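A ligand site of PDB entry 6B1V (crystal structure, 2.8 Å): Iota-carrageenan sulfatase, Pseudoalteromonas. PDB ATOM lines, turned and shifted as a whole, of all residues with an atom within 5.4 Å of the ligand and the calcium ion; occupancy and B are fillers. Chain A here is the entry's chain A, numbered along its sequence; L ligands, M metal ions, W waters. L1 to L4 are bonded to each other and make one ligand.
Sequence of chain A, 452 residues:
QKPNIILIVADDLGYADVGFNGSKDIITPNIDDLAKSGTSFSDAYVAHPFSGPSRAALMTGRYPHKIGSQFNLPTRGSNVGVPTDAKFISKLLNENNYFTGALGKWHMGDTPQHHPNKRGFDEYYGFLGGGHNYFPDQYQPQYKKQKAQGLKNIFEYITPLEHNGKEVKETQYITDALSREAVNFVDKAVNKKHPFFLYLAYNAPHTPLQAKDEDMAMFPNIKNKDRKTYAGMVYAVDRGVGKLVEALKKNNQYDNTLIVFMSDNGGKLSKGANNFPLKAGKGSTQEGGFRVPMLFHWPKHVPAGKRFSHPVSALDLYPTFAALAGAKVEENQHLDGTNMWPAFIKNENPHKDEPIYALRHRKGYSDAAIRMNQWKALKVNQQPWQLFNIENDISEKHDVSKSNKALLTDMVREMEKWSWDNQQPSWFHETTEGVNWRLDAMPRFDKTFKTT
The side-chain carboxylate (OD1) of Asp 11 is bound to the calcium ion (2.3 Å). The side-chain amide oxygen (OD1) of Asn 265 is bound to the calcium ion (2.3 Å). The calcium ion is bound by O7 of LG3 L3 (2.3 Å). OD1 of Asp 12 binds the calcium ion (2.4 Å). The calcium ion is bound by OD2 of Asp 264 (2.4 Å). OD1 of Asp 264 binds the calcium ion (2.9 Å).
Residues that only touch the ligand: Phe 50 (3.4 Å), Ser 51 (3.0 Å), His 107 (3.3 Å), Gly 130 (3.3 Å), Gly 131 (3.9 Å), Phe 155 (3.5 Å), Lys 268 (3.97 Å) and His 429 (3.5 Å). Hydrophobic or aromatic side chains that line the ligand: Phe 50, His 107, Phe 155, Tyr 157, His 206 and His 429. Within 4 Å of the ligand: Asp 11, Asp 12, Phe 50, Ser 51, Asn 72, Lys 105, His 107, Gly 130, Gly 131, Phe 155, Tyr 157, His 206, Thr 207, Asn 265, Lys 268, Lys 271, Lys 282, Gly 283, Arg 360 and His 429. The nearest printed residue that does not touch the ligand is Pro 49 (4.1 Å).
OG1 of Thr 207 sits at hydrogen-bond distance from O2 of LG2 L2, at 2.6 Å. The side-chain hydroxyl of Tyr 157 sits at hydrogen-bond distance from an oxygen (O5) of LG3 L3 (2.7 Å). ND2 of Asn 72 lies within hydrogen-bond range of O8 of LG3 L3, at 2.8 Å. The side-chain amino group of Lys 282 lies within salt-bridge range of an oxygen (O8) of LG3 L3. A ring nitrogen (NE2) of His 206 sits at hydrogen-bond distance from an oxygen (O3) of LG3 L3, at 3.0 Å. NH2 of Arg 360 lies within salt-bridge range of O5 of LG4 L4. O6 of LG3 L3 is in salt-bridge range of NZ of Lys 105 (3.1 Å). N of Gly 283 lies close to O6 of LG4 L4, 3.5 Å away. The side-chain amino group of Lys 271 is in salt-bridge range of an oxygen (O7) of LG2 L2, 3.8 Å away.
Ser 51 touches the calcium ion. Five residues have an atom within 4 Å of the calcium ion: Asp 11, Asp 12, Ser 51, Asp 264 and Asn 265. Along chain A the residues within 4 Å of the calcium ion span positions 11 to 265. The nearest printed residue that does not touch the calcium ion is His 206 (4.2 Å).
Water W2 bridges O2 of LG4 L4 (2.8 Å) and N of Asn 72 (3.1 Å).
The side-chain carboxylate (OD2) of Asp 12 lies within salt-bridge range of the side-chain amino group (NZ) of Lys 282 (3.1 Å). N of Gly 131 sits close to OH of Tyr 157 (3.5 Å). The backbone carbonyl oxygen of Asn 72 sits close to the backbone NH of His 429, 3.2 Å away. NZ of Lys 105 is in hydrogen-bond range of OG of Ser 51, at 2.9 Å. The side-chain hydroxyl (OG) of Ser 51 lies within hydrogen-bond range of the guanidinium group (NE) of Arg 55. The guanidinium group (NH2) of Arg 360 sits at hydrogen-bond distance from the backbone carbonyl oxygen (O) of Gly 283 (3.0 Å). The backbone carbonyl oxygen (O) of Gly 130 sits at hydrogen-bond distance from the side-chain amino group (NZ) of Lys 105 (2.8 Å). NH2 of Arg 362 lies within hydrogen-bond range of O of Gly 283 (3.2 Å).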
ATOM      1  N   ASP A  11      14.753   6.758   4.396  1.00  0.00           N
ATOM      2  CA  ASP A  11      14.528   8.049   5.030  1.00  0.00           C
ATOM      3  C   ASP A  11      13.045   8.113   5.385  1.00  0.00           C
ATOM      4  O   ASP A  11      12.212   8.011   4.495  1.00  0.00           O
ATOM      5  CB  ASP A  11      14.919   9.145   4.026  1.00  0.00           C
ATOM      6  CG  ASP A  11      14.980  10.556   4.630  1.00  0.00           C
ATOM      7  OD1 ASP A  11      14.702  10.712   5.841  1.00  0.00           O
ATOM      8  OD2 ASP A  11      15.284  11.500   3.865  1.00  0.00           O
ATOM      9  N   ASP A  12      12.740   8.252   6.671  1.00  0.00           N
ATOM     10  CA  ASP A  12      11.348   8.278   7.201  1.00  0.00           C
ATOM     11  C   ASP A  12      10.560   6.974   6.979  1.00  0.00           C
ATOM     12  O   ASP A  12       9.321   7.017   6.881  1.00  0.00           O
ATOM     13  CB  ASP A  12      10.527   9.471   6.631  1.00  0.00           C
ATOM     14  CG  ASP A  12      10.944  10.813   7.191  1.00  0.00           C
ATOM     15  OD1 ASP A  12      11.905  10.884   7.991  1.00  0.00           O
ATOM     16  OD2 ASP A  12      10.279  11.802   6.804  1.00  0.00           O
ATOM     17  N   PRO A  49      15.825  10.976  16.888  1.00  0.00           N
ATOM     18  CA  PRO A  49      14.606  10.640  16.135  1.00  0.00           C
ATOM     19  C   PRO A  49      14.356  11.425  14.849  1.00  0.00           C
ATOM     20  O   PRO A  49      13.215  11.446  14.369  1.00  0.00           O
ATOM     21  CB  PRO A  49      13.503  10.879  17.168  1.00  0.00           C
ATOM     22  CG  PRO A  49      14.044  11.956  18.015  1.00  0.00           C
ATOM     23  CD  PRO A  49      15.510  11.672  18.140  1.00  0.00           C
ATOM     24  N   PHE A  50      15.390  12.069  14.289  1.00  0.00           N
ATOM     25  CA  PHE A  50      15.303  12.578  12.917  1.00  0.00           C
ATOM     26  C   PHE A  50      16.677  12.659  12.233  1.00  0.00           C
ATOM     27  O   PHE A  50      17.701  12.407  12.872  1.00  0.00           O
ATOM     28  CB  PHE A  50      14.495  13.887  12.831  1.00  0.00           C
ATOM     29  CG  PHE A  50      15.071  15.032  13.620  1.00  0.00           C
ATOM     30  CD1 PHE A  50      16.166  15.732  13.152  1.00  0.00           C
ATOM     31  CD2 PHE A  50      14.459  15.467  14.784  1.00  0.00           C
ATOM     32  CE1 PHE A  50      16.678  16.821  13.858  1.00  0.00           C
ATOM     33  CE2 PHE A  50      14.954  16.554  15.494  1.00  0.00           C
ATOM     34  CZ  PHE A  50      16.073  17.236  15.035  1.00  0.00           C
ATOM     35  N   SER A  51      16.662  13.055  10.960  1.00  0.00           N
ATOM     36  CA  SER A  51      17.704  12.734   9.963  1.00  0.00           C
ATOM     37  C   SER A  51      19.148  13.133  10.271  1.00  0.00           C
ATOM     38  O   SER A  51      19.995  12.257  10.466  1.00  0.00           O
ATOM     39  CB  SER A  51      17.306  13.348   8.621  1.00  0.00           C
ATOM     40  OG  SER A  51      18.320  13.232   7.654  1.00  0.00           O
ATOM     41  N   GLY A  52      19.419  14.449  10.253  1.00  0.00           N
ATOM     42  CA  GLY A  52      20.772  14.977  10.292  1.00  0.00           C
ATOM     43  C   GLY A  52      21.573  14.397  11.431  1.00  0.00           C
ATOM     44  O   GLY A  52      22.582  13.732  11.194  1.00  0.00           O
ATOM     45  N   ARG A  55      22.135  10.561  11.179  1.00  0.00           N
ATOM     46  CA  ARG A  55      23.131  10.254  10.153  1.00  0.00           C
ATOM     47  C   ARG A  55      24.528  10.635  10.624  1.00  0.00           C
ATOM     48  O   ARG A  55      25.453   9.863  10.467  1.00  0.00           O
ATOM     49  CB  ARG A  55      22.808  10.960   8.834  1.00  0.00           C
ATOM     50  CG  ARG A  55      21.543  10.418   8.172  1.00  0.00           C
ATOM     51  CD  ARG A  55      20.904  11.403   7.213  1.00  0.00           C
ATOM     52  NE  ARG A  55      19.621  10.876   6.739  1.00  0.00           N
ATOM     53  CZ  ARG A  55      19.455   9.976   5.770  1.00  0.00           C
ATOM     54  NH1 ARG A  55      20.498   9.484   5.090  1.00  0.00           N
ATOM     55  NH2 ARG A  55      18.234   9.557   5.454  1.00  0.00           N
ATOM     56  N   ASN A  72      19.112  19.402  12.598  1.00  0.00           N
ATOM     57  CA  ASN A  72      19.262  19.404  11.137  1.00  0.00           C
ATOM     58  C   ASN A  72      19.929  20.700  10.750  1.00  0.00           C
ATOM     59  O   ASN A  72      19.735  21.732  11.406  1.00  0.00           O
ATOM     60  CB  ASN A  72      17.904  19.318  10.425  1.00  0.00           C
ATOM     61  CG  ASN A  72      17.326  17.911  10.380  1.00  0.00           C
ATOM     62  OD1 ASN A  72      17.955  16.932  10.774  1.00  0.00           O
ATOM     63  ND2 ASN A  72      16.110  17.833   9.865  1.00  0.00           N
ATOM     64  N   LYS A 105      21.257  10.744  -0.322  1.00  0.00           N
ATOM     65  CA  LYS A 105      21.140  11.818   0.637  1.00  0.00           C
ATOM     66  C   LYS A 105      22.387  11.904   1.510  1.00  0.00           C
ATOM     67  O   LYS A 105      22.934  10.882   1.934  1.00  0.00           O
ATOM     68  CB  LYS A 105      19.919  11.603   1.517  1.00  0.00           C
ATOM     69  CG  LYS A 105      19.615  12.711   2.522  1.00  0.00           C
ATOM     70  CD  LYS A 105      18.289  12.480   3.229  1.00  0.00           C
ATOM     71  CE  LYS A 105      18.199  13.323   4.492  1.00  0.00           C
ATOM     72  NZ  LYS A 105      16.855  13.374   5.118  1.00  0.00           N
ATOM     73  N   HIS A 107      23.039  15.293   3.893  1.00  0.00           N
ATOM     74  CA  HIS A 107      22.486  16.039   5.040  1.00  0.00           C
ATOM     75  C   HIS A 107      23.468  16.273   6.190  1.00  0.00           C
ATOM     76  O   HIS A 107      23.053  16.439   7.335  1.00  0.00           O
ATOM     77  CB  HIS A 107      21.205  15.351   5.541  1.00  0.00           C
ATOM     78  CG  HIS A 107      20.179  16.281   6.117  1.00  0.00           C
ATOM     79  ND1 HIS A 107      19.157  15.847   6.928  1.00  0.00           N
ATOM     80  CD2 HIS A 107      20.024  17.622   5.994  1.00  0.00           C
ATOM     81  CE1 HIS A 107      18.409  16.876   7.275  1.00  0.00           C
ATOM     82  NE2 HIS A 107      18.915  17.967   6.728  1.00  0.00           N
ATOM     83  N   GLY A 130      18.642  17.948   2.550  1.00  0.00           N
ATOM     84  CA  GLY A 130      17.700  17.133   3.355  1.00  0.00           C
ATOM     85  C   GLY A 130      16.763  16.185   2.602  1.00  0.00           C
ATOM     86  O   GLY A 130      16.178  15.267   3.190  1.00  0.00           O
ATOM     87  N   GLY A 131      16.622  16.400   1.303  1.00  0.00           N
ATOM     88  CA  GLY A 131      15.817  15.515   0.466  1.00  0.00           C
ATOM     89  C   GLY A 131      15.789  16.026  -0.958  1.00  0.00           C
ATOM     90  O   GLY A 131      16.547  16.937  -1.283  1.00  0.00           O
ATOM     91  N   PHE A 155      15.753  26.411  -3.459  1.00  0.00           N
ATOM     92  CA  PHE A 155      15.303  25.279  -2.654  1.00  0.00           C
ATOM     93  C   PHE A 155      16.047  24.024  -3.099  1.00  0.00           C
ATOM     94  O   PHE A 155      16.022  23.673  -4.278  1.00  0.00           O
ATOM     95  CB  PHE A 155      13.781  25.142  -2.851  1.00  0.00           C
ATOM     96  CG  PHE A 155      13.135  24.032  -2.070  1.00  0.00           C
ATOM     97  CD1 PHE A 155      13.452  23.791  -0.733  1.00  0.00           C
ATOM     98  CD2 PHE A 155      12.136  23.249  -2.668  1.00  0.00           C
ATOM     99  CE1 PHE A 155      12.823  22.776  -0.016  1.00  0.00           C
ATOM    100  CE2 PHE A 155      11.494  22.232  -1.956  1.00  0.00           C
ATOM    101  CZ  PHE A 155      11.844  21.996  -0.627  1.00  0.00           C
ATOM    102  N   GLU A 156      16.725  23.368  -2.174  1.00  0.00           N
ATOM    103  CA  GLU A 156      17.687  22.317  -2.577  1.00  0.00           C
ATOM    104  C   GLU A 156      17.036  21.069  -3.195  1.00  0.00           C
ATOM    105  O   GLU A 156      17.697  20.325  -3.889  1.00  0.00           O
ATOM    106  CB  GLU A 156      18.686  21.979  -1.444  1.00  0.00           C
ATOM    107  CG  GLU A 156      18.322  20.843  -0.486  1.00  0.00           C
ATOM    108  CD  GLU A 156      18.635  21.215   0.983  1.00  0.00           C
ATOM    109  OE1 GLU A 156      19.740  21.742   1.268  1.00  0.00           O
ATOM    110  OE2 GLU A 156      17.781  20.970   1.870  1.00  0.00           O
ATOM    111  N   TYR A 157      15.727  20.907  -2.995  1.00  0.00           N
ATOM    112  CA  TYR A 157      14.972  19.759  -3.553  1.00  0.00           C
ATOM    113  C   TYR A 157      14.869  19.737  -5.085  1.00  0.00           C
ATOM    114  O   TYR A 157      14.570  18.688  -5.649  1.00  0.00           O
ATOM    115  CB  TYR A 157      13.560  19.668  -2.961  1.00  0.00           C
ATOM    116  CG  TYR A 157      13.484  19.009  -1.596  1.00  0.00           C
ATOM    117  CD1 TYR A 157      12.646  17.917  -1.354  1.00  0.00           C
ATOM    118  CD2 TYR A 157      14.264  19.472  -0.528  1.00  0.00           C
ATOM    119  CE1 TYR A 157      12.579  17.313  -0.113  1.00  0.00           C
ATOM    120  CE2 TYR A 157      14.206  18.870   0.728  1.00  0.00           C
ATOM    121  CZ  TYR A 157      13.368  17.791   0.927  1.00  0.00           C
ATOM    122  OH  TYR A 157      13.329  17.207   2.170  1.00  0.00           O
ATOM    123  N   HIS A 206      10.587   9.551   2.106  1.00  0.00           N
ATOM    124  CA  HIS A 206      10.498  10.906   2.646  1.00  0.00           C
ATOM    125  C   HIS A 206       9.757  11.772   1.651  1.00  0.00           C
ATOM    126  O   HIS A 206       9.769  11.499   0.458  1.00  0.00           O
ATOM    127  CB  HIS A 206      11.918  11.471   2.865  1.00  0.00           C
ATOM    128  CG  HIS A 206      11.963  12.768   3.597  1.00  0.00           C
ATOM    129  ND1 HIS A 206      11.636  13.967   3.010  1.00  0.00           N
ATOM    130  CD2 HIS A 206      12.376  13.065   4.855  1.00  0.00           C
ATOM    131  CE1 HIS A 206      11.815  14.939   3.879  1.00  0.00           C
ATOM    132  NE2 HIS A 206      12.266  14.428   5.010  1.00  0.00           N
ATOM    133  N   THR A 207       9.137  12.813   2.170  1.00  0.00           N
ATOM    134  CA  THR A 207       8.406  13.765   1.356  1.00  0.00           C
ATOM    135  C   THR A 207       9.353  14.410   0.330  1.00  0.00           C
ATOM    136  O   THR A 207      10.567  14.438   0.571  1.00  0.00           O
ATOM    137  CB  THR A 207       7.727  14.848   2.229  1.00  0.00           C
ATOM    138  OG1 THR A 207       8.689  15.410   3.148  1.00  0.00           O
ATOM    139  CG2 THR A 207       6.566  14.238   2.987  1.00  0.00           C
ATOM    140  N   PRO A 208       8.840  14.910  -0.794  1.00  0.00           N
ATOM    141  CA  PRO A 208       7.409  14.929  -1.132  1.00  0.00           C
ATOM    142  C   PRO A 208       6.924  13.583  -1.655  1.00  0.00           C
ATOM    143  O   PRO A 208       7.692  12.845  -2.273  1.00  0.00           O
ATOM    144  CB  PRO A 208       7.335  15.993  -2.216  1.00  0.00           C
ATOM    145  CG  PRO A 208       8.643  15.854  -2.925  1.00  0.00           C
ATOM    146  CD  PRO A 208       9.666  15.360  -1.931  1.00  0.00           C
ATOM    147  N   ASP A 264      16.556   5.864   8.935  1.00  0.00           N
ATOM    148  CA  ASP A 264      17.269   6.917   9.656  1.00  0.00           C
ATOM    149  C   ASP A 264      16.502   7.349  10.919  1.00  0.00           C
ATOM    150  O   ASP A 264      17.110   7.788  11.906  1.00  0.00           O
ATOM    151  CB  ASP A 264      17.592   8.126   8.749  1.00  0.00           C
ATOM    152  CG  ASP A 264      16.372   8.976   8.380  1.00  0.00           C
ATOM    153  OD1 ASP A 264      15.240   8.450   8.312  1.00  0.00           O
ATOM    154  OD2 ASP A 264      16.538  10.190   8.154  1.00  0.00           O
ATOM    155  N   ASN A 265      15.176   7.235  10.877  1.00  0.00           N
ATOM    156  CA  ASN A 265      14.315   7.576  11.991  1.00  0.00           C
ATOM    157  C   ASN A 265      12.942   6.912  11.798  1.00  0.00           C
ATOM    158  O   ASN A 265      12.733   6.198  10.830  1.00  0.00           O
ATOM    159  CB  ASN A 265      14.204   9.104  12.131  1.00  0.00           C
ATOM    160  CG  ASN A 265      13.699   9.788  10.867  1.00  0.00           C
ATOM    161  OD1 ASN A 265      14.421  10.585  10.264  1.00  0.00           O
ATOM    162  ND2 ASN A 265      12.469   9.488  10.467  1.00  0.00           N
ATOM    163  N   LYS A 268       6.685   9.190   9.582  1.00  0.00           N
ATOM    164  CA  LYS A 268       5.821  10.327   9.898  1.00  0.00           C
ATOM    165  C   LYS A 268       4.384   9.985   9.509  1.00  0.00           C
ATOM    166  O   LYS A 268       4.079   9.837   8.334  1.00  0.00           O
ATOM    167  CB  LYS A 268       6.299  11.589   9.174  1.00  0.00           C
ATOM    168  CG  LYS A 268       5.560  12.852   9.621  1.00  0.00           C
ATOM    169  CD  LYS A 268       6.240  14.142   9.185  1.00  0.00           C
ATOM    170  CE  LYS A 268       5.656  15.359   9.897  1.00  0.00           C
ATOM    171  NZ  LYS A 268       6.495  16.574   9.694  1.00  0.00           N
ATOM    172  N   LYS A 271       2.479  11.832   6.740  1.00  0.00           N
ATOM    173  CA  LYS A 271       3.013  11.645   5.372  1.00  0.00           C
ATOM    174  C   LYS A 271       3.102  10.178   4.956  1.00  0.00           C
ATOM    175  O   LYS A 271       4.129   9.744   4.401  1.00  0.00           O
ATOM    176  CB  LYS A 271       4.391  12.301   5.254  1.00  0.00           C
ATOM    177  CG  LYS A 271       4.436  13.749   5.690  1.00  0.00           C
ATOM    178  CD  LYS A 271       3.544  14.665   4.853  1.00  0.00           C
ATOM    179  CE  LYS A 271       3.697  16.096   5.354  1.00  0.00           C
ATOM    180  NZ  LYS A 271       2.778  16.967   4.601  1.00  0.00           N
ATOM    181  N   LYS A 282       7.952   9.968  13.761  1.00  0.00           N
ATOM    182  CA  LYS A 282       9.148  10.770  13.511  1.00  0.00           C
ATOM    183  C   LYS A 282       9.362  11.895  14.531  1.00  0.00           C
ATOM    184  O   LYS A 282       8.430  12.626  14.834  1.00  0.00           O
ATOM    185  CB  LYS A 282       9.070  11.372  12.093  1.00  0.00           C
ATOM    186  CG  LYS A 282      10.316  12.120  11.634  1.00  0.00           C
ATOM    187  CD  LYS A 282      10.059  12.831  10.320  1.00  0.00           C
ATOM    188  CE  LYS A 282      11.299  13.541   9.836  1.00  0.00           C
ATOM    189  NZ  LYS A 282      11.053  14.255   8.570  1.00  0.00           N
ATOM    190  N   GLY A 283      10.571  12.015  15.044  1.00  0.00           N
ATOM    191  CA  GLY A 283      10.938  13.128  15.941  1.00  0.00           C
ATOM    192  C   GLY A 283      10.630  12.941  17.417  1.00  0.00           C
ATOM    193  O   GLY A 283      11.108  13.726  18.226  1.00  0.00           O
ATOM    194  N   ARG A 360      15.968  14.880  22.303  1.00  0.00           N
ATOM    195  CA  ARG A 360      15.537  15.739  21.196  1.00  0.00           C
ATOM    196  C   ARG A 360      14.992  17.024  21.766  1.00  0.00           C
ATOM    197  O   ARG A 360      14.133  17.007  22.638  1.00  0.00           O
ATOM    198  CB  ARG A 360      14.483  15.042  20.353  1.00  0.00           C
ATOM    199  CG  ARG A 360      13.924  15.877  19.193  1.00  0.00           C
ATOM    200  CD  ARG A 360      12.583  16.517  19.533  1.00  0.00           C
ATOM    201  NE  ARG A 360      12.319  17.618  18.611  1.00  0.00           N
ATOM    202  CZ  ARG A 360      11.819  17.514  17.381  1.00  0.00           C
ATOM    203  NH1 ARG A 360      11.651  18.615  16.659  1.00  0.00           N
ATOM    204  NH2 ARG A 360      11.493  16.325  16.853  1.00  0.00           N
ATOM    205  N   ARG A 362      13.200  20.820  21.974  1.00  0.00           N
ATOM    206  CA  ARG A 362      11.983  21.519  21.568  1.00  0.00           C
ATOM    207  C   ARG A 362      12.076  22.969  22.056  1.00  0.00           C
ATOM    208  O   ARG A 362      13.157  23.403  22.499  1.00  0.00           O
ATOM    209  CB  ARG A 362      10.779  20.775  22.130  1.00  0.00           C
ATOM    210  CG  ARG A 362      10.706  19.335  21.607  1.00  0.00           C
ATOM    211  CD  ARG A 362       9.280  18.821  21.475  1.00  0.00           C
ATOM    212  NE  ARG A 362       9.201  17.459  20.952  1.00  0.00           N
ATOM    213  CZ  ARG A 362       9.092  17.106  19.674  1.00  0.00           C
ATOM    214  NH1 ARG A 362       9.047  18.028  18.714  1.00  0.00           N
ATOM    215  NH2 ARG A 362       9.022  15.815  19.342  1.00  0.00           N
ATOM    216  N   HIS A 429      18.227  24.325  12.626  1.00  0.00           N
ATOM    217  CA  HIS A 429      17.594  24.139  11.306  1.00  0.00           C
ATOM    218  C   HIS A 429      16.951  25.435  10.747  1.00  0.00           C
ATOM    219  O   HIS A 429      16.683  25.516   9.553  1.00  0.00           O
ATOM    220  CB  HIS A 429      16.593  22.949  11.327  1.00  0.00           C
ATOM    221  CG  HIS A 429      15.185  23.339  11.618  1.00  0.00           C
ATOM    222  ND1 HIS A 429      14.761  23.723  12.877  1.00  0.00           N
ATOM    223  CD2 HIS A 429      14.085  23.367  10.831  1.00  0.00           C
ATOM    224  CE1 HIS A 429      13.467  23.995  12.832  1.00  0.00           C
ATOM    225  NE2 HIS A 429      13.033  23.788  11.602  1.00  0.00           N
ATOM    226  N   GLU A 433      15.094  29.306  15.669  1.00  0.00           N
ATOM    227  CA  GLU A 433      15.313  28.206  16.605  1.00  0.00           C
ATOM    228  C   GLU A 433      16.554  28.441  17.482  1.00  0.00           C
ATOM    229  O   GLU A 433      16.539  28.139  18.671  1.00  0.00           O
ATOM    230  CB  GLU A 433      15.441  26.880  15.844  1.00  0.00           C
ATOM    231  CG  GLU A 433      15.236  25.647  16.701  1.00  0.00           C
ATOM    232  CD  GLU A 433      15.365  24.329  15.952  1.00  0.00           C
ATOM    233  OE1 GLU A 433      16.142  24.258  14.978  1.00  0.00           O
ATOM    234  OE2 GLU A 433      14.676  23.375  16.356  1.00  0.00           O
HETATM  235  C1  LIG L   1       8.467  25.553   0.583  1.00  0.00           C
HETATM  236  C2  LIG L   1       8.196  24.428   1.591  1.00  0.00           C
HETATM  237  C3  LIG L   1       8.499  23.024   1.080  1.00  0.00           C
HETATM  238  C4  LIG L   1       7.997  22.872  -0.348  1.00  0.00           C
HETATM  239  C5  LIG L   1       8.611  23.989  -1.207  1.00  0.00           C
HETATM  240  C6  LIG L   1       8.417  23.901  -2.734  1.00  0.00           C
HETATM  241  O1  LIG L   1       7.702  26.709   0.951  1.00  0.00           O
HETATM  242  O2  LIG L   1       8.976  24.650   2.766  1.00  0.00           O
HETATM  243  O3  LIG L   1       7.844  22.095   1.974  1.00  0.00           O
HETATM  244  O4  LIG L   1       6.559  22.941  -0.352  1.00  0.00           O
HETATM  245  O5  LIG L   1       8.075  25.229  -0.754  1.00  0.00           O
HETATM  246  O6  LIG L   1       7.648  22.748  -3.126  1.00  0.00           O
HETATM  247  S1  LIG L   1       5.649  21.692  -0.449  1.00  0.00           S
HETATM  248  O7  LIG L   1       6.199  20.694  -1.327  1.00  0.00           O
HETATM  249  O8  LIG L   1       4.187  22.188  -0.961  1.00  0.00           O
HETATM  250  O9  LIG L   1       5.436  21.115   0.854  1.00  0.00           O
HETATM  251  C1  LG2 L   2       8.442  20.773   2.104  1.00  0.00           C
HETATM  252  C2  LG2 L   2       7.518  19.898   2.989  1.00  0.00           C
HETATM  253  C3  LG2 L   2       8.254  18.675   3.513  1.00  0.00           C
HETATM  254  C4  LG2 L   2       9.446  19.137   4.314  1.00  0.00           C
HETATM  255  C5  LG2 L   2      10.320  19.551   3.152  1.00  0.00           C
HETATM  256  C6  LG2 L   2      10.110  18.413   2.167  1.00  0.00           C
HETATM  257  O1  LG2 L   2       7.017  20.645   4.103  1.00  0.00           O
HETATM  258  O2  LG2 L   2       8.775  17.924   2.406  1.00  0.00           O
HETATM  259  O3  LG2 L   2       9.883  18.026   5.101  1.00  0.00           O
HETATM  260  O4  LG2 L   2       9.807  20.768   2.578  1.00  0.00           O
HETATM  261  O5  LG2 L   2       5.487  21.204   5.884  1.00  0.00           O
HETATM  262  O6  LG2 L   2       5.961  18.781   5.615  1.00  0.00           O
HETATM  263  O7  LG2 L   2       4.625  20.196   3.994  1.00  0.00           O
HETATM  264  S1  LG2 L   2       5.762  20.227   4.874  1.00  0.00           S
HETATM  265  C1  LG3 L   3      11.024  18.314   5.896  1.00  0.00           C
HETATM  266  C2  LG3 L   3      10.797  17.650   7.233  1.00  0.00           C
HETATM  267  C3  LG3 L   3      11.993  17.907   8.135  1.00  0.00           C
HETATM  268  C4  LG3 L   3      13.284  17.380   7.489  1.00  0.00           C
HETATM  269  C5  LG3 L   3      13.416  18.034   6.103  1.00  0.00           C
HETATM  270  C6  LG3 L   3      14.603  17.521   5.307  1.00  0.00           C
HETATM  271  O1  LG3 L   3       9.611  18.157   7.802  1.00  0.00           O
HETATM  272  O2  LG3 L   3      11.751  17.310   9.404  1.00  0.00           O
HETATM  273  O3  LG3 L   3      13.228  15.934   7.436  1.00  0.00           O
HETATM  274  O4  LG3 L   3      12.228  17.824   5.313  1.00  0.00           O
HETATM  275  O5  LG3 L   3      14.712  18.334   4.134  1.00  0.00           O
HETATM  276  S1  LG3 L   3      14.359  15.074   8.027  1.00  0.00           S
HETATM  277  O6  LG3 L   3      15.512  15.285   7.184  1.00  0.00           O
HETATM  278  O7  LG3 L   3      14.026  13.482   8.072  1.00  0.00           O
HETATM  279  O8  LG3 L   3      14.604  15.502   9.374  1.00  0.00           O
HETATM  280  C1  LG4 L   4      12.358  18.073  10.458  1.00  0.00           C
HETATM  281  C2  LG4 L   4      12.282  17.305  11.775  1.00  0.00           C
HETATM  282  C3  LG4 L   4      12.626  18.269  12.926  1.00  0.00           C
HETATM  283  C4  LG4 L   4      11.654  19.438  12.963  1.00  0.00           C
HETATM  284  C5  LG4 L   4      12.148  20.130  11.735  1.00  0.00           C
HETATM  285  C6  LG4 L   4      13.657  20.115  11.975  1.00  0.00           C
HETATM  286  O1  LG4 L   4      10.953  16.792  11.843  1.00  0.00           O
HETATM  287  O2  LG4 L   4      13.905  18.876  12.658  1.00  0.00           O
HETATM  288  O3  LG4 L   4      11.817  20.321  14.081  1.00  0.00           O
HETATM  289  O4  LG4 L   4      11.717  19.345  10.622  1.00  0.00           O
HETATM  290  O5  LG4 L   4      10.085  16.895  14.120  1.00  0.00           O
HETATM  291  O6  LG4 L   4      11.332  15.004  13.451  1.00  0.00           O
HETATM  292  O7  LG4 L   4       9.031  15.267  12.536  1.00  0.00           O
HETATM  293  S1  LG4 L   4      10.391  16.008  13.029  1.00  0.00           S
HETATM  294 CA    CA M   1      14.306  11.167   8.021  1.00  0.00          CA
HETATM  295  O   HOH W   1      15.014  20.213   8.437  1.00  0.00           O
HETATM  296  O   HOH W   2      16.276  20.097  13.590  1.00  0.00           O
